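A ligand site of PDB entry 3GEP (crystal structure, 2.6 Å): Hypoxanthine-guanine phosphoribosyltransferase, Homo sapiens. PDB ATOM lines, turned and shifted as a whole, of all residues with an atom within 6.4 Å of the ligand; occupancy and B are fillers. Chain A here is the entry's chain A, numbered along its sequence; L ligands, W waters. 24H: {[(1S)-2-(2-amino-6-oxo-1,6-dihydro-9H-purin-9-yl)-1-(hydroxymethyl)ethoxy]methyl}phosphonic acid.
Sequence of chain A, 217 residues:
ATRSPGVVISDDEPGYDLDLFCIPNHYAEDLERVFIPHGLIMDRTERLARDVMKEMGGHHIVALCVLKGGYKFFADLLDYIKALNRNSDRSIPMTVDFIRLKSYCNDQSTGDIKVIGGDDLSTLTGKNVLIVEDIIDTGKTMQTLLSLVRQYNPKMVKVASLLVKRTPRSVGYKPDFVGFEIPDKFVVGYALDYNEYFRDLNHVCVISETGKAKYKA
O of Lys 185 lies within hydrogen-bond range of NZ of Lys 165, 3.2 Å away.
The side-chain carboxylate (OD2) of Asp 137 lies within salt-bridge range of the guanidinium group (NH2) of Arg 169 (2.4 Å).
The side-chain hydroxyl (OG1) of Thr 138 lies close to the backbone NH (N) of Lys 140 (3.3 Å).
The side-chain hydroxyl of Thr 141 lies within hydrogen-bond range of the backbone carbonyl oxygen of Thr 110, at 2.9 Å.
The side-chain amino group of Lys 165 is in salt-bridge range of the side-chain carboxylate of Asp 137, at 3.9 Å.
The backbone carbonyl oxygen (O) of Ile 136 is in hydrogen-bond range of the backbone NH (N) of Lys 165, 2.9 Å away.
O of Lys 185 sits close to O6 of the ligand (3.4 Å).
Merely in contact with the ligand: Asp 107 (3.4 Å), Thr 110 (3.4 Å), Ile 135 (3.6 Å), Ile 136 (3.8 Å), Lys 140 (3.6 Å), Phe 186 (3.3 Å) and Leu 192 (3.7 Å).
Hydrophobic or aromatic side chains within 4 Å of the ligand: Ile 135, Phe 186, Val 187 and Leu 192.
15 residues have an atom within 4 Å of the ligand: Lys 68, Asp 107, Thr 110, Ile 135, Ile 136, Asp 137, Thr 138, Gly 139, Lys 140, Thr 141, Lys 165, Lys 185, Phe 186, Val 187 and Leu 192.
Water W2 lies within hydrogen-bond range of OAF of the ligand, OD2 of Asp 137, OD1 of Asp 107 and NH2 of Arg 169.
Water W1 lies within hydrogen-bond range of an oxygen (OAE) of the ligand (2.7 Å), the backbone NH (N) of Met 142 (3.0 Å) and the backbone NH (N) of Thr 141 (3.4 Å).
Water W4 lies within hydrogen-bond range of the side-chain amino group (NZ) of Lys 68, the side-chain carboxylate (OE1) of Glu 133, an oxygen (OAD) of the ligand and the backbone carbonyl oxygen (O) of Ile 135.
Water W3 bridges the backbone carbonyl oxygen of Asp 193 and a nitrogen (N2) of the ligand.
OAE of the ligand is in hydrogen-bond range of N of Gly 139.
OG1 of Thr 138 lies within hydrogen-bond range of OAF of the ligand, 2.8 Å away.
An oxygen (O6) of the ligand sits at hydrogen-bond distance from the backbone NH of Val 187 (3.0 Å).
The backbone NH of Thr 141 sits at hydrogen-bond distance from an oxygen (OAC) of the ligand (3.1 Å).
OG1 of Thr 141 lies within hydrogen-bond range of OAC of the ligand.
NZ of Lys 68 is in hydrogen-bond range of OAD of the ligand, at 2.8 Å.
OAF of the ligand lies within hydrogen-bond range of N of Thr 138 (3.1 Å).
NZ of Lys 165 sits at hydrogen-bond distance from O6 of the ligand (2.6 Å).
The backbone NH (N) of Asp 137 lies within hydrogen-bond range of an oxygen (OAE) of the ligand (2.8 Å).
The backbone carbonyl oxygen of Val 187 lies within hydrogen-bond range of a nitrogen (N1) of the ligand, 2.8 Å away.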
ATOM      1  N   LYS A  68     -20.038 -31.479 -12.205  1.00  0.00           N
ATOM      2  CA  LYS A  68     -21.462 -31.469 -11.918  1.00  0.00           C
ATOM      3  C   LYS A  68     -22.200 -31.074 -13.195  1.00  0.00           C
ATOM      4  O   LYS A  68     -22.567 -31.925 -14.009  1.00  0.00           O
ATOM      5  CB  LYS A  68     -21.788 -30.503 -10.780  1.00  0.00           C
ATOM      6  CG  LYS A  68     -21.171 -30.892  -9.429  1.00  0.00           C
ATOM      7  CD  LYS A  68     -21.730 -30.020  -8.322  1.00  0.00           C
ATOM      8  CE  LYS A  68     -21.382 -30.566  -6.942  1.00  0.00           C
ATOM      9  NZ  LYS A  68     -21.678 -29.580  -5.864  1.00  0.00           N
ATOM     10  N   ASP A 107     -29.873 -29.215  -2.916  1.00  0.00           N
ATOM     11  CA  ASP A 107     -29.142 -28.000  -2.568  1.00  0.00           C
ATOM     12  C   ASP A 107     -29.525 -27.505  -1.164  1.00  0.00           C
ATOM     13  O   ASP A 107     -29.512 -26.306  -0.875  1.00  0.00           O
ATOM     14  CB  ASP A 107     -29.368 -26.912  -3.625  1.00  0.00           C
ATOM     15  CG  ASP A 107     -28.155 -26.018  -3.836  1.00  0.00           C
ATOM     16  OD1 ASP A 107     -27.096 -26.262  -3.222  1.00  0.00           O
ATOM     17  OD2 ASP A 107     -28.258 -25.055  -4.641  1.00  0.00           O
ATOM     18  N   THR A 110     -26.327 -30.681   0.422  1.00  0.00           N
ATOM     19  CA  THR A 110     -25.249 -30.762  -0.570  1.00  0.00           C
ATOM     20  C   THR A 110     -24.020 -31.530  -0.037  1.00  0.00           C
ATOM     21  O   THR A 110     -23.155 -31.959  -0.819  1.00  0.00           O
ATOM     22  CB  THR A 110     -24.817 -29.351  -1.064  1.00  0.00           C
ATOM     23  OG1 THR A 110     -25.791 -28.381  -0.674  1.00  0.00           O
ATOM     24  CG2 THR A 110     -24.676 -29.336  -2.575  1.00  0.00           C
ATOM     25  N   GLY A 111     -23.978 -31.694   1.287  1.00  0.00           N
ATOM     26  CA  GLY A 111     -22.930 -32.466   1.950  1.00  0.00           C
ATOM     27  C   GLY A 111     -22.954 -33.948   1.615  1.00  0.00           C
ATOM     28  O   GLY A 111     -21.934 -34.607   1.667  1.00  0.00           O
ATOM     29  N   GLU A 133     -12.870 -26.775  -8.494  1.00  0.00           N
ATOM     30  CA  GLU A 133     -14.289 -26.485  -8.296  1.00  0.00           C
ATOM     31  C   GLU A 133     -14.614 -25.132  -8.948  1.00  0.00           C
ATOM     32  O   GLU A 133     -13.757 -24.253  -9.013  1.00  0.00           O
ATOM     33  CB  GLU A 133     -14.569 -26.421  -6.797  1.00  0.00           C
ATOM     34  CG  GLU A 133     -16.028 -26.218  -6.392  1.00  0.00           C
ATOM     35  CD  GLU A 133     -16.957 -27.307  -6.922  1.00  0.00           C
ATOM     36  OE1 GLU A 133     -17.477 -28.088  -6.098  1.00  0.00           O
ATOM     37  OE2 GLU A 133     -17.163 -27.380  -8.156  1.00  0.00           O
ATOM     38  N   ASP A 134     -15.855 -24.959  -9.404  1.00  0.00           N
ATOM     39  CA  ASP A 134     -16.277 -23.667  -9.959  1.00  0.00           C
ATOM     40  C   ASP A 134     -16.895 -22.721  -8.940  1.00  0.00           C
ATOM     41  O   ASP A 134     -16.637 -21.510  -8.969  1.00  0.00           O
ATOM     42  CB  ASP A 134     -17.171 -23.832 -11.197  1.00  0.00           C
ATOM     43  CG  ASP A 134     -18.429 -24.667 -10.939  1.00  0.00           C
ATOM     44  OD1 ASP A 134     -18.728 -25.042  -9.786  1.00  0.00           O
ATOM     45  OD2 ASP A 134     -19.119 -24.955 -11.933  1.00  0.00           O
ATOM     46  N   ILE A 135     -17.695 -23.260  -8.032  1.00  0.00           N
ATOM     47  CA  ILE A 135     -18.321 -22.468  -6.975  1.00  0.00           C
ATOM     48  C   ILE A 135     -18.389 -23.212  -5.644  1.00  0.00           C
ATOM     49  O   ILE A 135     -18.723 -24.408  -5.591  1.00  0.00           O
ATOM     50  CB  ILE A 135     -19.729 -21.924  -7.405  1.00  0.00           C
ATOM     51  CG1 ILE A 135     -20.284 -20.960  -6.349  1.00  0.00           C
ATOM     52  CG2 ILE A 135     -20.695 -23.079  -7.752  1.00  0.00           C
ATOM     53  CD1 ILE A 135     -21.338 -20.004  -6.866  1.00  0.00           C
ATOM     54  N   ILE A 136     -18.056 -22.500  -4.578  1.00  0.00           N
ATOM     55  CA  ILE A 136     -18.314 -22.960  -3.226  1.00  0.00           C
ATOM     56  C   ILE A 136     -19.309 -22.014  -2.551  1.00  0.00           C
ATOM     57  O   ILE A 136     -19.138 -20.796  -2.580  1.00  0.00           O
ATOM     58  CB  ILE A 136     -16.992 -23.082  -2.418  1.00  0.00           C
ATOM     59  CG1 ILE A 136     -16.252 -24.348  -2.878  1.00  0.00           C
ATOM     60  CG2 ILE A 136     -17.263 -23.129  -0.900  1.00  0.00           C
ATOM     61  CD1 ILE A 136     -14.802 -24.428  -2.436  1.00  0.00           C
ATOM     62  N   ASP A 137     -20.368 -22.611  -1.995  1.00  0.00           N
ATOM     63  CA  ASP A 137     -21.427 -21.887  -1.299  1.00  0.00           C
ATOM     64  C   ASP A 137     -21.358 -22.179   0.219  1.00  0.00           C
ATOM     65  O   ASP A 137     -20.678 -21.474   0.955  1.00  0.00           O
ATOM     66  CB  ASP A 137     -22.778 -22.238  -1.928  1.00  0.00           C
ATOM     67  CG  ASP A 137     -23.946 -21.497  -1.305  1.00  0.00           C
ATOM     68  OD1 ASP A 137     -23.782 -20.330  -0.894  1.00  0.00           O
ATOM     69  OD2 ASP A 137     -25.043 -22.076  -1.222  1.00  0.00           O
ATOM     70  N   THR A 138     -22.048 -23.233   0.691  1.00  0.00           N
ATOM     71  CA  THR A 138     -21.943 -23.651   2.089  1.00  0.00           C
ATOM     72  C   THR A 138     -20.602 -24.313   2.358  1.00  0.00           C
ATOM     73  O   THR A 138     -20.118 -24.314   3.493  1.00  0.00           O
ATOM     74  CB  THR A 138     -23.070 -24.638   2.520  1.00  0.00           C
ATOM     75  OG1 THR A 138     -22.953 -25.866   1.785  1.00  0.00           O
ATOM     76  CG2 THR A 138     -24.451 -24.061   2.310  1.00  0.00           C
ATOM     77  N   GLY A 139     -20.009 -24.903   1.316  1.00  0.00           N
ATOM     78  CA  GLY A 139     -18.746 -25.638   1.441  1.00  0.00           C
ATOM     79  C   GLY A 139     -18.894 -27.092   1.882  1.00  0.00           C
ATOM     80  O   GLY A 139     -17.890 -27.782   2.031  1.00  0.00           O
ATOM     81  N   LYS A 140     -20.136 -27.558   2.076  1.00  0.00           N
ATOM     82  CA  LYS A 140     -20.404 -28.937   2.539  1.00  0.00           C
ATOM     83  C   LYS A 140     -19.958 -30.009   1.542  1.00  0.00           C
ATOM     84  O   LYS A 140     -19.357 -31.021   1.939  1.00  0.00           O
ATOM     85  CB  LYS A 140     -21.886 -29.132   2.864  1.00  0.00           C
ATOM     86  CG  LYS A 140     -22.386 -28.401   4.088  1.00  0.00           C
ATOM     87  CD  LYS A 140     -23.820 -28.795   4.340  1.00  0.00           C
ATOM     88  CE  LYS A 140     -24.505 -27.862   5.306  1.00  0.00           C
ATOM     89  NZ  LYS A 140     -25.942 -27.721   4.906  1.00  0.00           N
ATOM     90  N   THR A 141     -20.266 -29.790   0.259  1.00  0.00           N
ATOM     91  CA  THR A 141     -19.879 -30.694  -0.821  1.00  0.00           C
ATOM     92  C   THR A 141     -18.381 -30.954  -0.790  1.00  0.00           C
ATOM     93  O   THR A 141     -17.952 -32.111  -0.821  1.00  0.00           O
ATOM     94  CB  THR A 141     -20.251 -30.095  -2.204  1.00  0.00           C
ATOM     95  OG1 THR A 141     -21.676 -29.952  -2.286  1.00  0.00           O
ATOM     96  CG2 THR A 141     -19.770 -31.001  -3.345  1.00  0.00           C
ATOM     97  N   MET A 142     -17.608 -29.885  -0.730  1.00  0.00           N
ATOM     98  CA  MET A 142     -16.149 -29.958  -0.798  1.00  0.00           C
ATOM     99  C   MET A 142     -15.524 -30.644   0.412  1.00  0.00           C
ATOM    100  O   MET A 142     -14.619 -31.463   0.249  1.00  0.00           O
ATOM    101  CB  MET A 142     -15.543 -28.567  -0.999  1.00  0.00           C
ATOM    102  CG  MET A 142     -14.056 -28.572  -1.278  1.00  0.00           C
ATOM    103  SD  MET A 142     -13.522 -29.728  -2.570  1.00  0.00           S
ATOM    104  CE  MET A 142     -14.279 -29.010  -4.018  1.00  0.00           C
ATOM    105  N   LYS A 165     -18.575 -17.969  -2.116  1.00  0.00           N
ATOM    106  CA  LYS A 165     -19.688 -17.138  -1.708  1.00  0.00           C
ATOM    107  C   LYS A 165     -19.562 -16.747  -0.239  1.00  0.00           C
ATOM    108  O   LYS A 165     -19.353 -17.599   0.637  1.00  0.00           O
ATOM    109  CB  LYS A 165     -20.990 -17.891  -1.939  1.00  0.00           C
ATOM    110  CG  LYS A 165     -22.065 -17.114  -2.614  1.00  0.00           C
ATOM    111  CD  LYS A 165     -22.894 -18.049  -3.488  1.00  0.00           C
ATOM    112  CE  LYS A 165     -24.353 -17.914  -3.129  1.00  0.00           C
ATOM    113  NZ  LYS A 165     -25.241 -18.613  -4.089  1.00  0.00           N
ATOM    114  N   ARG A 169     -24.071 -19.137   5.806  1.00  0.00           N
ATOM    115  CA  ARG A 169     -24.357 -20.571   5.651  1.00  0.00           C
ATOM    116  C   ARG A 169     -23.088 -21.419   5.431  1.00  0.00           C
ATOM    117  O   ARG A 169     -23.138 -22.644   5.410  1.00  0.00           O
ATOM    118  CB  ARG A 169     -25.360 -20.791   4.514  1.00  0.00           C
ATOM    119  CG  ARG A 169     -26.837 -20.544   4.875  1.00  0.00           C
ATOM    120  CD  ARG A 169     -27.705 -20.235   3.638  1.00  0.00           C
ATOM    121  NE  ARG A 169     -27.482 -21.197   2.557  1.00  0.00           N
ATOM    122  CZ  ARG A 169     -26.843 -20.933   1.423  1.00  0.00           C
ATOM    123  NH1 ARG A 169     -26.355 -19.728   1.154  1.00  0.00           N
ATOM    124  NH2 ARG A 169     -26.700 -21.886   0.525  1.00  0.00           N
ATOM    125  N   ILE A 182     -17.517 -13.509  -3.588  1.00  0.00           N
ATOM    126  CA  ILE A 182     -18.680 -12.795  -4.113  1.00  0.00           C
ATOM    127  C   ILE A 182     -19.766 -12.619  -3.071  1.00  0.00           C
ATOM    128  O   ILE A 182     -19.771 -13.326  -2.066  1.00  0.00           O
ATOM    129  CB  ILE A 182     -19.220 -13.475  -5.395  1.00  0.00           C
ATOM    130  CG1 ILE A 182     -19.507 -14.969  -5.151  1.00  0.00           C
ATOM    131  CG2 ILE A 182     -18.225 -13.279  -6.554  1.00  0.00           C
ATOM    132  CD1 ILE A 182     -20.536 -15.546  -6.076  1.00  0.00           C
ATOM    133  N   LYS A 185     -25.404 -14.090  -3.374  1.00  0.00           N
ATOM    134  CA  LYS A 185     -26.467 -14.051  -4.392  1.00  0.00           C
ATOM    135  C   LYS A 185     -26.307 -15.222  -5.350  1.00  0.00           C
ATOM    136  O   LYS A 185     -25.215 -15.766  -5.496  1.00  0.00           O
ATOM    137  CB  LYS A 185     -26.418 -12.726  -5.170  1.00  0.00           C
ATOM    138  CG  LYS A 185     -27.095 -11.568  -4.442  1.00  0.00           C
ATOM    139  CD  LYS A 185     -26.537 -10.243  -4.901  1.00  0.00           C
ATOM    140  CE  LYS A 185     -27.143  -9.082  -4.111  1.00  0.00           C
ATOM    141  NZ  LYS A 185     -26.332  -7.825  -4.244  1.00  0.00           N
ATOM    142  N   PHE A 186     -27.405 -15.636  -5.971  1.00  0.00           N
ATOM    143  CA  PHE A 186     -27.388 -16.807  -6.835  1.00  0.00           C
ATOM    144  C   PHE A 186     -26.913 -16.403  -8.220  1.00  0.00           C
ATOM    145  O   PHE A 186     -27.581 -15.643  -8.944  1.00  0.00           O
ATOM    146  CB  PHE A 186     -28.750 -17.518  -6.894  1.00  0.00           C
ATOM    147  CG  PHE A 186     -28.665 -18.917  -7.444  1.00  0.00           C
ATOM    148  CD1 PHE A 186     -28.466 -19.998  -6.596  1.00  0.00           C
ATOM    149  CD2 PHE A 186     -28.754 -19.152  -8.820  1.00  0.00           C
ATOM    150  CE1 PHE A 186     -28.362 -21.291  -7.103  1.00  0.00           C
ATOM    151  CE2 PHE A 186     -28.635 -20.429  -9.331  1.00  0.00           C
ATOM    152  CZ  PHE A 186     -28.457 -21.503  -8.483  1.00  0.00           C
ATOM    153  N   VAL A 187     -25.739 -16.901  -8.582  1.00  0.00           N
ATOM    154  CA  VAL A 187     -25.087 -16.533  -9.832  1.00  0.00           C
ATOM    155  C   VAL A 187     -25.153 -17.631 -10.879  1.00  0.00           C
ATOM    156  O   VAL A 187     -25.183 -18.829 -10.568  1.00  0.00           O
ATOM    157  CB  VAL A 187     -23.620 -16.065  -9.618  1.00  0.00           C
ATOM    158  CG1 VAL A 187     -23.589 -14.714  -8.877  1.00  0.00           C
ATOM    159  CG2 VAL A 187     -22.797 -17.110  -8.866  1.00  0.00           C
ATOM    160  N   VAL A 188     -25.168 -17.202 -12.130  1.00  0.00           N
ATOM    161  CA  VAL A 188     -25.121 -18.088 -13.284  1.00  0.00           C
ATOM    162  C   VAL A 188     -24.143 -17.499 -14.301  1.00  0.00           C
ATOM    163  O   VAL A 188     -23.726 -16.350 -14.163  1.00  0.00           O
ATOM    164  CB  VAL A 188     -26.511 -18.225 -13.954  1.00  0.00           C
ATOM    165  CG1 VAL A 188     -27.471 -19.017 -13.066  1.00  0.00           C
ATOM    166  CG2 VAL A 188     -27.074 -16.853 -14.291  1.00  0.00           C
ATOM    167  N   LEU A 192     -21.434 -21.696 -14.835  1.00  0.00           N
ATOM    168  CA  LEU A 192     -22.622 -22.070 -14.068  1.00  0.00           C
ATOM    169  C   LEU A 192     -23.899 -22.035 -14.906  1.00  0.00           C
ATOM    170  O   LEU A 192     -24.289 -20.987 -15.416  1.00  0.00           O
ATOM    171  CB  LEU A 192     -22.753 -21.197 -12.829  1.00  0.00           C
ATOM    172  CG  LEU A 192     -21.491 -21.194 -11.944  1.00  0.00           C
ATOM    173  CD1 LEU A 192     -21.539 -20.057 -10.950  1.00  0.00           C
ATOM    174  CD2 LEU A 192     -21.335 -22.528 -11.256  1.00  0.00           C
ATOM    175  N   ASP A 193     -24.531 -23.200 -15.041  1.00  0.00           N
ATOM    176  CA  ASP A 193     -25.827 -23.287 -15.706  1.00  0.00           C
ATOM    177  C   ASP A 193     -26.971 -23.288 -14.691  1.00  0.00           C
ATOM    178  O   ASP A 193     -26.779 -23.642 -13.517  1.00  0.00           O
ATOM    179  CB  ASP A 193     -25.909 -24.497 -16.657  1.00  0.00           C
ATOM    180  CG  ASP A 193     -25.958 -25.835 -15.932  1.00  0.00           C
ATOM    181  OD1 ASP A 193     -24.896 -26.325 -15.501  1.00  0.00           O
ATOM    182  OD2 ASP A 193     -27.058 -26.423 -15.821  1.00  0.00           O
ATOM    183  N   TYR A 194     -28.144 -22.858 -15.139  1.00  0.00           N
ATOM    184  CA  TYR A 194     -29.377 -23.010 -14.372  1.00  0.00           C
ATOM    185  C   TYR A 194     -30.280 -23.890 -15.209  1.00  0.00           C
ATOM    186  O   TYR A 194     -30.832 -23.452 -16.223  1.00  0.00           O
ATOM    187  CB  TYR A 194     -30.032 -21.662 -14.098  1.00  0.00           C
ATOM    188  CG  TYR A 194     -31.167 -21.705 -13.092  1.00  0.00           C
ATOM    189  CD1 TYR A 194     -30.908 -21.845 -11.726  1.00  0.00           C
ATOM    190  CD2 TYR A 194     -32.496 -21.580 -13.492  1.00  0.00           C
ATOM    191  CE1 TYR A 194     -31.931 -21.880 -10.793  1.00  0.00           C
ATOM    192  CE2 TYR A 194     -33.538 -21.611 -12.568  1.00  0.00           C
ATOM    193  CZ  TYR A 194     -33.239 -21.762 -11.218  1.00  0.00           C
ATOM    194  OH  TYR A 194     -34.250 -21.789 -10.285  1.00  0.00           O
HETATM  195  C4  24H L   1     -24.991 -22.563  -6.600  1.00  0.00           C
HETATM  196  C5  24H L   1     -24.923 -21.252  -6.125  1.00  0.00           C
HETATM  197  C6  24H L   1     -24.944 -20.191  -7.030  1.00  0.00           C
HETATM  198  C8  24H L   1     -24.883 -22.632  -4.432  1.00  0.00           C
HETATM  199  O6  24H L   1     -24.880 -19.010  -6.614  1.00  0.00           O
HETATM  200  N7  24H L   1     -24.853 -21.325  -4.782  1.00  0.00           N
HETATM  201  N1  24H L   1     -25.019 -20.452  -8.349  1.00  0.00           N
HETATM  202  C2  24H L   1     -25.069 -21.738  -8.807  1.00  0.00           C
HETATM  203  N2  24H L   1     -25.164 -21.964 -10.142  1.00  0.00           N
HETATM  204  N3  24H L   1     -25.059 -22.779  -7.943  1.00  0.00           N
HETATM  205  N9  24H L   1     -24.942 -23.387  -5.531  1.00  0.00           N
HETATM  206  CAJ 24H L   1     -25.014 -24.849  -5.555  1.00  0.00           C
HETATM  207  CAS 24H L   1     -23.752 -25.616  -5.145  1.00  0.00           C
HETATM  208  CAH 24H L   1     -22.885 -25.766  -6.379  1.00  0.00           C
HETATM  209  OAD 24H L   1     -22.909 -27.167  -6.688  1.00  0.00           O
HETATM  210  OAN 24H L   1     -23.007 -25.148  -3.993  1.00  0.00           O
HETATM  211  CAI 24H L   1     -22.340 -26.272  -3.386  1.00  0.00           C
HETATM  212  PAU 24H L   1     -22.023 -26.148  -1.595  1.00  0.00           P
HETATM  213  OAE 24H L   1     -20.736 -25.369  -1.470  1.00  0.00           O
HETATM  214  OAF 24H L   1     -23.243 -25.485  -1.006  1.00  0.00           O
HETATM  215  OAC 24H L   1     -21.879 -27.567  -1.103  1.00  0.00           O
HETATM  216  O   HOH W   1     -18.799 -27.212  -1.484  1.00  0.00           O
HETATM  217  O   HOH W   2     -25.527 -24.576  -1.338  1.00  0.00           O
HETATM  218  O   HOH W   3     -24.573 -24.292 -12.066  1.00  0.00           O
HETATM  219  O   HOH W   4     -20.127 -27.448  -6.468  1.00  0.00           O
